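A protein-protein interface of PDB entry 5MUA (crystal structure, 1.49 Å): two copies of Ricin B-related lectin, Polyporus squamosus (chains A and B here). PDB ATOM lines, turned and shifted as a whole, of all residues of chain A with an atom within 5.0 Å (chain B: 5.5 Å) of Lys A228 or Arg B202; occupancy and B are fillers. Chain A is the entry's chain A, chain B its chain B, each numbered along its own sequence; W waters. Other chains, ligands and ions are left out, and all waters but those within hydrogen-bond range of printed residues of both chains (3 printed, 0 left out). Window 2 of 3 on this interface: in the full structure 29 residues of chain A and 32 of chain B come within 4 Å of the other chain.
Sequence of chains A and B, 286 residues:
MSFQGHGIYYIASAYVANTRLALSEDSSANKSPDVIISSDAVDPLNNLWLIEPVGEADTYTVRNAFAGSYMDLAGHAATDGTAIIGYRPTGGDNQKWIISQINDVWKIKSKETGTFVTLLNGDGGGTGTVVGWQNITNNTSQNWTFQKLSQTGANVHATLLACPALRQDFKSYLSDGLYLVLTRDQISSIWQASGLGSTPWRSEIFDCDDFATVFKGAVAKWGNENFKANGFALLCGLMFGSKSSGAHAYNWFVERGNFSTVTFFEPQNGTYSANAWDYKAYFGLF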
ATOM      1  N   ARG A  63      35.462  22.865 -28.724  1.00  0.00           N
ATOM      2  CA  ARG A  63      34.100  23.262 -29.064  1.00  0.00           C
ATOM      3  C   ARG A  63      34.013  24.734 -29.354  1.00  0.00           C
ATOM      4  O   ARG A  63      34.624  25.559 -28.627  1.00  0.00           O
ATOM      5  CB  ARG A  63      33.203  22.919 -27.912  1.00  0.00           C
ATOM      6  CG  ARG A  63      31.703  23.033 -28.169  1.00  0.00           C
ATOM      7  CD  ARG A  63      30.823  22.888 -26.896  1.00  0.00           C
ATOM      8  NE  ARG A  63      29.436  22.691 -27.302  1.00  0.00           N
ATOM      9  CZ  ARG A  63      28.397  22.532 -26.479  1.00  0.00           C
ATOM     10  NH1 ARG A  63      28.577  22.571 -25.179  1.00  0.00           N
ATOM     11  NH2 ARG A  63      27.206  22.383 -26.951  1.00  0.00           N
ATOM     12  N   ALA A  65      32.601  27.910 -28.885  1.00  0.00           N
ATOM     13  CA  ALA A  65      31.732  28.536 -27.832  1.00  0.00           C
ATOM     14  C   ALA A  65      30.454  29.191 -28.441  1.00  0.00           C
ATOM     15  O   ALA A  65      29.300  29.019 -27.903  1.00  0.00           O
ATOM     16  CB  ALA A  65      32.528  29.545 -27.035  1.00  0.00           C
ATOM     17  N   PHE A  66      30.629  29.890 -29.551  1.00  0.00           N
ATOM     18  CA  PHE A  66      29.529  30.634 -30.198  1.00  0.00           C
ATOM     19  C   PHE A  66      28.501  29.627 -30.775  1.00  0.00           C
ATOM     20  O   PHE A  66      27.310  29.649 -30.439  1.00  0.00           O
ATOM     21  CB  PHE A  66      30.106  31.518 -31.324  1.00  0.00           C
ATOM     22  CG  PHE A  66      29.085  32.253 -32.115  1.00  0.00           C
ATOM     23  CD1 PHE A  66      28.549  33.435 -31.605  1.00  0.00           C
ATOM     24  CD2 PHE A  66      28.673  31.805 -33.375  1.00  0.00           C
ATOM     25  CE1 PHE A  66      27.640  34.135 -32.354  1.00  0.00           C
ATOM     26  CE2 PHE A  66      27.712  32.502 -34.092  1.00  0.00           C
ATOM     27  CZ  PHE A  66      27.224  33.679 -33.591  1.00  0.00           C
ATOM     28  N   ALA A  67      28.959  28.774 -31.685  1.00  0.00           N
ATOM     29  CA  ALA A  67      28.063  27.954 -32.447  1.00  0.00           C
ATOM     30  C   ALA A  67      27.673  26.704 -31.743  1.00  0.00           C
ATOM     31  O   ALA A  67      26.706  26.041 -32.131  1.00  0.00           O
ATOM     32  CB  ALA A  67      28.705  27.613 -33.805  1.00  0.00           C
ATOM     33  N   GLY A  68      28.423  26.284 -30.749  1.00  0.00           N
ATOM     34  CA  GLY A  68      28.098  25.023 -30.016  1.00  0.00           C
ATOM     35  C   GLY A  68      28.597  23.724 -30.674  1.00  0.00           C
ATOM     36  O   GLY A  68      28.669  22.657 -30.020  1.00  0.00           O
ATOM     37  N   GLY A 223      25.528  36.752 -22.762  1.00  0.00           N
ATOM     38  CA  GLY A 223      26.135  35.449 -22.896  1.00  0.00           C
ATOM     39  C   GLY A 223      25.147  34.434 -23.396  1.00  0.00           C
ATOM     40  O   GLY A 223      25.462  33.644 -24.249  1.00  0.00           O
ATOM     41  N   ASN A 224      23.942  34.445 -22.811  1.00  0.00           N
ATOM     42  CA  ASN A 224      22.948  33.467 -23.188  1.00  0.00           C
ATOM     43  C   ASN A 224      22.528  33.663 -24.628  1.00  0.00           C
ATOM     44  O   ASN A 224      22.297  32.692 -25.340  1.00  0.00           O
ATOM     45  CB  ASN A 224      21.737  33.607 -22.290  1.00  0.00           C
ATOM     46  CG  ASN A 224      20.664  32.643 -22.672  1.00  0.00           C
ATOM     47  OD1 ASN A 224      20.843  31.443 -22.648  1.00  0.00           O
ATOM     48  ND2 ASN A 224      19.547  33.190 -23.023  1.00  0.00           N
ATOM     49  N   ASN A 226      24.337  34.827 -27.027  1.00  0.00           N
ATOM     50  CA  ASN A 226      25.441  34.709 -28.033  1.00  0.00           C
ATOM     51  C   ASN A 226      26.211  33.449 -28.048  1.00  0.00           C
ATOM     52  O   ASN A 226      26.944  33.212 -29.039  1.00  0.00           O
ATOM     53  CB  ASN A 226      26.403  35.856 -27.844  1.00  0.00           C
ATOM     54  CG  ASN A 226      25.867  37.113 -28.432  1.00  0.00           C
ATOM     55  OD1 ASN A 226      25.883  37.250 -29.661  1.00  0.00           O
ATOM     56  ND2 ASN A 226      25.304  37.983 -27.615  1.00  0.00           N
ATOM     57  N   PHE A 227      26.113  32.645 -26.998  1.00  0.00           N
ATOM     58  CA  PHE A 227      26.921  31.387 -26.931  1.00  0.00           C
ATOM     59  C   PHE A 227      26.035  30.168 -26.794  1.00  0.00           C
ATOM     60  O   PHE A 227      25.326  29.999 -25.794  1.00  0.00           O
ATOM     61  CB  PHE A 227      27.921  31.446 -25.775  1.00  0.00           C
ATOM     62  CG  PHE A 227      28.884  32.556 -25.891  1.00  0.00           C
ATOM     63  CD1 PHE A 227      29.968  32.457 -26.751  1.00  0.00           C
ATOM     64  CD2 PHE A 227      28.769  33.696 -25.121  1.00  0.00           C
ATOM     65  CE1 PHE A 227      30.861  33.503 -26.874  1.00  0.00           C
ATOM     66  CE2 PHE A 227      29.647  34.739 -25.254  1.00  0.00           C
ATOM     67  CZ  PHE A 227      30.731  34.640 -26.123  1.00  0.00           C
ATOM     68  N   LYS A 228      26.103  29.301 -27.782  1.00  0.00           N
ATOM     69  CA  LYS A 228      25.357  28.048 -27.794  1.00  0.00           C
ATOM     70  C   LYS A 228      25.992  26.917 -27.000  1.00  0.00           C
ATOM     71  O   LYS A 228      25.288  25.969 -26.616  1.00  0.00           O
ATOM     72  CB  LYS A 228      25.080  27.554 -29.225  1.00  0.00           C
ATOM     73  CG  LYS A 228      24.115  28.453 -29.995  1.00  0.00           C
ATOM     74  CD  LYS A 228      23.947  28.092 -31.472  1.00  0.00           C
ATOM     75  CE  LYS A 228      23.354  26.707 -31.659  1.00  0.00           C
ATOM     76  NZ  LYS A 228      22.029  26.413 -31.002  1.00  0.00           N
ATOM     77  N   ALA A 229      27.305  27.010 -26.749  1.00  0.00           N
ATOM     78  CA  ALA A 229      27.965  26.086 -25.864  1.00  0.00           C
ATOM     79  C   ALA A 229      27.563  26.371 -24.437  1.00  0.00           C
ATOM     80  O   ALA A 229      27.098  27.477 -24.126  1.00  0.00           O
ATOM     81  CB  ALA A 229      29.459  26.177 -25.953  1.00  0.00           C
ATOM     82  N   ASN A 230      27.678  25.346 -23.609  1.00  0.00           N
ATOM     83  CA  ASN A 230      27.504  25.478 -22.142  1.00  0.00           C
ATOM     84  C   ASN A 230      28.860  25.275 -21.465  1.00  0.00           C
ATOM     85  O   ASN A 230      29.900  25.164 -22.160  1.00  0.00           O
ATOM     86  CB  ASN A 230      26.456  24.459 -21.658  1.00  0.00           C
ATOM     87  CG  ASN A 230      26.915  23.062 -21.714  1.00  0.00           C
ATOM     88  OD1 ASN A 230      27.977  22.721 -22.300  1.00  0.00           O
ATOM     89  ND2 ASN A 230      26.123  22.195 -21.115  1.00  0.00           N
ATOM     90  N   PRO B 200      15.714  28.317 -21.836  1.00  0.00           N
ATOM     91  CA  PRO B 200      16.190  27.020 -21.321  1.00  0.00           C
ATOM     92  C   PRO B 200      17.355  27.137 -20.290  1.00  0.00           C
ATOM     93  O   PRO B 200      18.195  28.029 -20.443  1.00  0.00           O
ATOM     94  CB  PRO B 200      16.702  26.292 -22.619  1.00  0.00           C
ATOM     95  CG  PRO B 200      16.054  26.987 -23.783  1.00  0.00           C
ATOM     96  CD  PRO B 200      15.760  28.432 -23.299  1.00  0.00           C
ATOM     97  N   TRP B 201      17.408  26.212 -19.339  1.00  0.00           N
ATOM     98  CA  TRP B 201      18.467  26.112 -18.410  1.00  0.00           C
ATOM     99  C   TRP B 201      19.668  25.573 -19.146  1.00  0.00           C
ATOM    100  O   TRP B 201      19.580  24.558 -19.819  1.00  0.00           O
ATOM    101  CB  TRP B 201      18.130  25.220 -17.238  1.00  0.00           C
ATOM    102  CG  TRP B 201      19.140  25.016 -16.196  1.00  0.00           C
ATOM    103  CD1 TRP B 201      19.192  25.667 -14.975  1.00  0.00           C
ATOM    104  CD2 TRP B 201      20.235  24.084 -16.163  1.00  0.00           C
ATOM    105  NE1 TRP B 201      20.236  25.245 -14.230  1.00  0.00           N
ATOM    106  CE2 TRP B 201      20.926  24.296 -14.932  1.00  0.00           C
ATOM    107  CE3 TRP B 201      20.733  23.122 -17.047  1.00  0.00           C
ATOM    108  CZ2 TRP B 201      22.058  23.576 -14.567  1.00  0.00           C
ATOM    109  CZ3 TRP B 201      21.880  22.424 -16.695  1.00  0.00           C
ATOM    110  CH2 TRP B 201      22.516  22.639 -15.447  1.00  0.00           C
ATOM    111  N   ARG B 202      20.814  26.233 -18.965  1.00  0.00           N
ATOM    112  CA  ARG B 202      22.065  25.670 -19.522  1.00  0.00           C
ATOM    113  C   ARG B 202      23.147  25.860 -18.514  1.00  0.00           C
ATOM    114  O   ARG B 202      23.334  26.984 -17.934  1.00  0.00           O
ATOM    115  CB  ARG B 202      22.410  26.265 -20.866  1.00  0.00           C
ATOM    116  CG  ARG B 202      21.279  26.209 -21.901  1.00  0.00           C
ATOM    117  CD  ARG B 202      21.738  26.581 -23.328  1.00  0.00           C
ATOM    118  NE  ARG B 202      21.880  28.051 -23.463  1.00  0.00           N
ATOM    119  CZ  ARG B 202      22.945  28.682 -23.926  1.00  0.00           C
ATOM    120  NH1 ARG B 202      24.013  27.976 -24.368  1.00  0.00           N
ATOM    121  NH2 ARG B 202      22.970  29.996 -23.992  1.00  0.00           N
ATOM    122  N   SER B 203      23.923  24.800 -18.330  1.00  0.00           N
ATOM    123  CA  SER B 203      24.914  24.747 -17.302  1.00  0.00           C
ATOM    124  C   SER B 203      25.945  25.859 -17.447  1.00  0.00           C
ATOM    125  O   SER B 203      26.443  26.069 -18.537  1.00  0.00           O
ATOM    126  CB  SER B 203      25.594  23.391 -17.300  1.00  0.00           C
ATOM    127  OG  SER B 203      26.413  23.282 -16.156  1.00  0.00           O
ATOM    128  N   GLU B 204      26.223  26.548 -16.344  1.00  0.00           N
ATOM    129  CA  GLU B 204      27.154  27.749 -16.262  1.00  0.00           C
ATOM    130  C   GLU B 204      26.714  28.984 -17.008  1.00  0.00           C
ATOM    131  O   GLU B 204      26.665  30.098 -16.430  1.00  0.00           O
ATOM    132  CB  GLU B 204      28.582  27.369 -16.616  1.00  0.00           C
ATOM    133  CG  GLU B 204      29.309  26.502 -15.562  1.00  0.00           C
ATOM    134  CD  GLU B 204      28.864  25.041 -15.546  1.00  0.00           C
ATOM    135  OE1 GLU B 204      28.597  24.481 -16.637  1.00  0.00           O
ATOM    136  OE2 GLU B 204      28.826  24.483 -14.424  1.00  0.00           O
ATOM    137  N   ILE B 205      26.383  28.858 -18.290  1.00  0.00           N
ATOM    138  CA  ILE B 205      26.159  29.975 -19.152  1.00  0.00           C
ATOM    139  C   ILE B 205      24.782  30.649 -18.897  1.00  0.00           C
ATOM    140  O   ILE B 205      24.640  31.832 -19.052  1.00  0.00           O
ATOM    141  CB  ILE B 205      26.360  29.511 -20.604  1.00  0.00           C
ATOM    142  CG1 ILE B 205      26.494  30.680 -21.558  1.00  0.00           C
ATOM    143  CG2 ILE B 205      25.252  28.533 -21.076  1.00  0.00           C
ATOM    144  CD1 ILE B 205      27.621  31.682 -21.273  1.00  0.00           C
ATOM    145  N   PHE B 206      23.819  29.845 -18.497  1.00  0.00           N
ATOM    146  CA  PHE B 206      22.548  30.367 -18.020  1.00  0.00           C
ATOM    147  C   PHE B 206      21.857  29.366 -17.104  1.00  0.00           C
ATOM    148  O   PHE B 206      20.909  28.702 -17.440  1.00  0.00           O
ATOM    149  CB  PHE B 206      21.646  30.823 -19.154  1.00  0.00           C
ATOM    150  CG  PHE B 206      20.759  31.942 -18.722  1.00  0.00           C
ATOM    151  CD1 PHE B 206      21.233  33.261 -18.730  1.00  0.00           C
ATOM    152  CD2 PHE B 206      19.497  31.684 -18.275  1.00  0.00           C
ATOM    153  CE1 PHE B 206      20.464  34.335 -18.317  1.00  0.00           C
ATOM    154  CE2 PHE B 206      18.717  32.764 -17.813  1.00  0.00           C
ATOM    155  CZ  PHE B 206      19.187  34.067 -17.843  1.00  0.00           C
ATOM    156  N   ASP B 207      22.367  29.325 -15.880  1.00  0.00           N
ATOM    157  CA  ASP B 207      22.008  28.403 -14.838  1.00  0.00           C
ATOM    158  C   ASP B 207      21.434  29.159 -13.593  1.00  0.00           C
ATOM    159  O   ASP B 207      21.046  30.333 -13.726  1.00  0.00           O
ATOM    160  CB  ASP B 207      23.048  27.335 -14.602  1.00  0.00           C
ATOM    161  CG  ASP B 207      24.401  27.885 -14.153  1.00  0.00           C
ATOM    162  OD1 ASP B 207      24.558  29.153 -14.169  1.00  0.00           O
ATOM    163  OD2 ASP B 207      25.216  27.056 -13.659  1.00  0.00           O
ATOM    164  N   PHE B 211      19.436  32.915 -13.582  1.00  0.00           N
ATOM    165  CA  PHE B 211      18.006  33.107 -13.385  1.00  0.00           C
ATOM    166  C   PHE B 211      17.766  34.008 -12.198  1.00  0.00           C
ATOM    167  O   PHE B 211      16.952  34.939 -12.339  1.00  0.00           O
ATOM    168  CB  PHE B 211      17.283  31.789 -13.176  1.00  0.00           C
ATOM    169  CG  PHE B 211      17.076  31.005 -14.454  1.00  0.00           C
ATOM    170  CD1 PHE B 211      15.962  31.228 -15.252  1.00  0.00           C
ATOM    171  CD2 PHE B 211      18.036  30.086 -14.887  1.00  0.00           C
ATOM    172  CE1 PHE B 211      15.790  30.561 -16.437  1.00  0.00           C
ATOM    173  CE2 PHE B 211      17.862  29.384 -16.068  1.00  0.00           C
ATOM    174  CZ  PHE B 211      16.738  29.651 -16.864  1.00  0.00           C
HETATM  175  O   HOH W   1      25.682  34.146 -19.841  1.00  0.00           O
HETATM  176  O   HOH W   2      19.267  29.246 -22.665  1.00  0.00           O
HETATM  177  O   HOH W   3      24.392  24.758 -24.273  1.00  0.00           O
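Printed residues of chain A that touch a printed residue of chain B: Asn A224, Phe A227, Lys A228, Ala A229 and Asn A230. Of the 9 printed residues of chain B, 4 touch a printed residue of chain A. Printed residues of chain B that touch a printed residue of chain A: Arg B202, Ser B203, Ile B205 and Phe B206. Hydrophobic or aromatic side chains of chain B that line the printed part of chain A: Ile B205 and Phe B206. Among the printed residues, 8 pairs touch across the chains. Among the printed residues, no Asp or Glu carboxylate lies within 4 Å of a Lys or Arg side-chain nitrogen of the other chain.
No position is printed for both chains. Of the 8 pairs that touch across the chains among the printed residues, none has its exchanged pair printed and touching as well.
N of Asp B207 sits at hydrogen-bond distance from O of Arg B202 (3.3 Å). The side-chain hydroxyl of Ser B203 is in hydrogen-bond range of the side-chain carboxylate of Glu B204, at 2.5 Å. NH1 of Arg A63 lies within hydrogen-bond range of OD1 of Asn A230, at 2.9 Å. The backbone carbonyl oxygen of Ala A65 sits at hydrogen-bond distance from the backbone NH of Ala A229. O of Ala A65 sits at hydrogen-bond distance from N of Lys A228, 3.2 Å away. O of Phe A66 sits at hydrogen-bond distance from N of Lys A228, at 2.9 Å.
Among the printed residues, merely in contact across the chains: Asn A224 with Phe B206 (3.6 Å), Ala A229 with Ile B205 (3.7 Å), Asn A230 with Ser B203 (3.5 Å) and Asn A230 with Ile B205 (3.9 Å).
Of the printed residues of chain B, Lys A228 touches Arg B202. Of chain A, only Asn A224, Phe A227, Lys A228 and Ala A229 come within 4 Å of Arg B202. Of the printed residues of chain B, Ala A229 touches Arg B202 (3.1 Å) and Ile B205 (3.7 Å). Printed residues of chain B within 4 Å of Asn A224: Arg B202 (2.9 Å) and Phe B206 (3.6 Å). Of the printed residues of chain A, Ile B205 touches Ala A229 and Asn A230. Of the printed residues of chain B, Phe A227 touches Arg B202 (2.8 Å). Of the printed residues of chain A, Ser B203 touches Asn A230 (3.5 Å). Phe B211 touches none of the printed residues of chain A. Pro B200 touches none of the printed residues of chain A. The nearest printed residue of chain B that does not touch Lys A228 is Ile B205 (6.1 Å).
The guanidinium group (NH1) of Arg B202 sits at hydrogen-bond distance from the backbone carbonyl oxygen (O) of Lys A228 (3.3 Å). OD1 of Asn A224 sits at hydrogen-bond distance from NH2 of Arg B202 (2.9 Å). O of Ala A229 sits at hydrogen-bond distance from NH1 of Arg B202 (3.1 Å). O of Phe A227 sits at hydrogen-bond distance from NH1 of Arg B202 (2.8 Å).
Water W1 bridges the backbone carbonyl oxygen (O) of Ile B205 (2.7 Å) and the backbone NH (N) of Asn A224 (3.5 Å). Water W2 lies within hydrogen-bond range of OD1 of Asn A224 (2.7 Å), O of Pro B200 (2.8 Å) and NE of Arg B202 (3.0 Å). Water W3 lies within hydrogen-bond range of the backbone carbonyl oxygen (O) of Lys A228, the guanidinium group (NH1) of Arg B202 and the backbone NH (N) of Asn A230.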
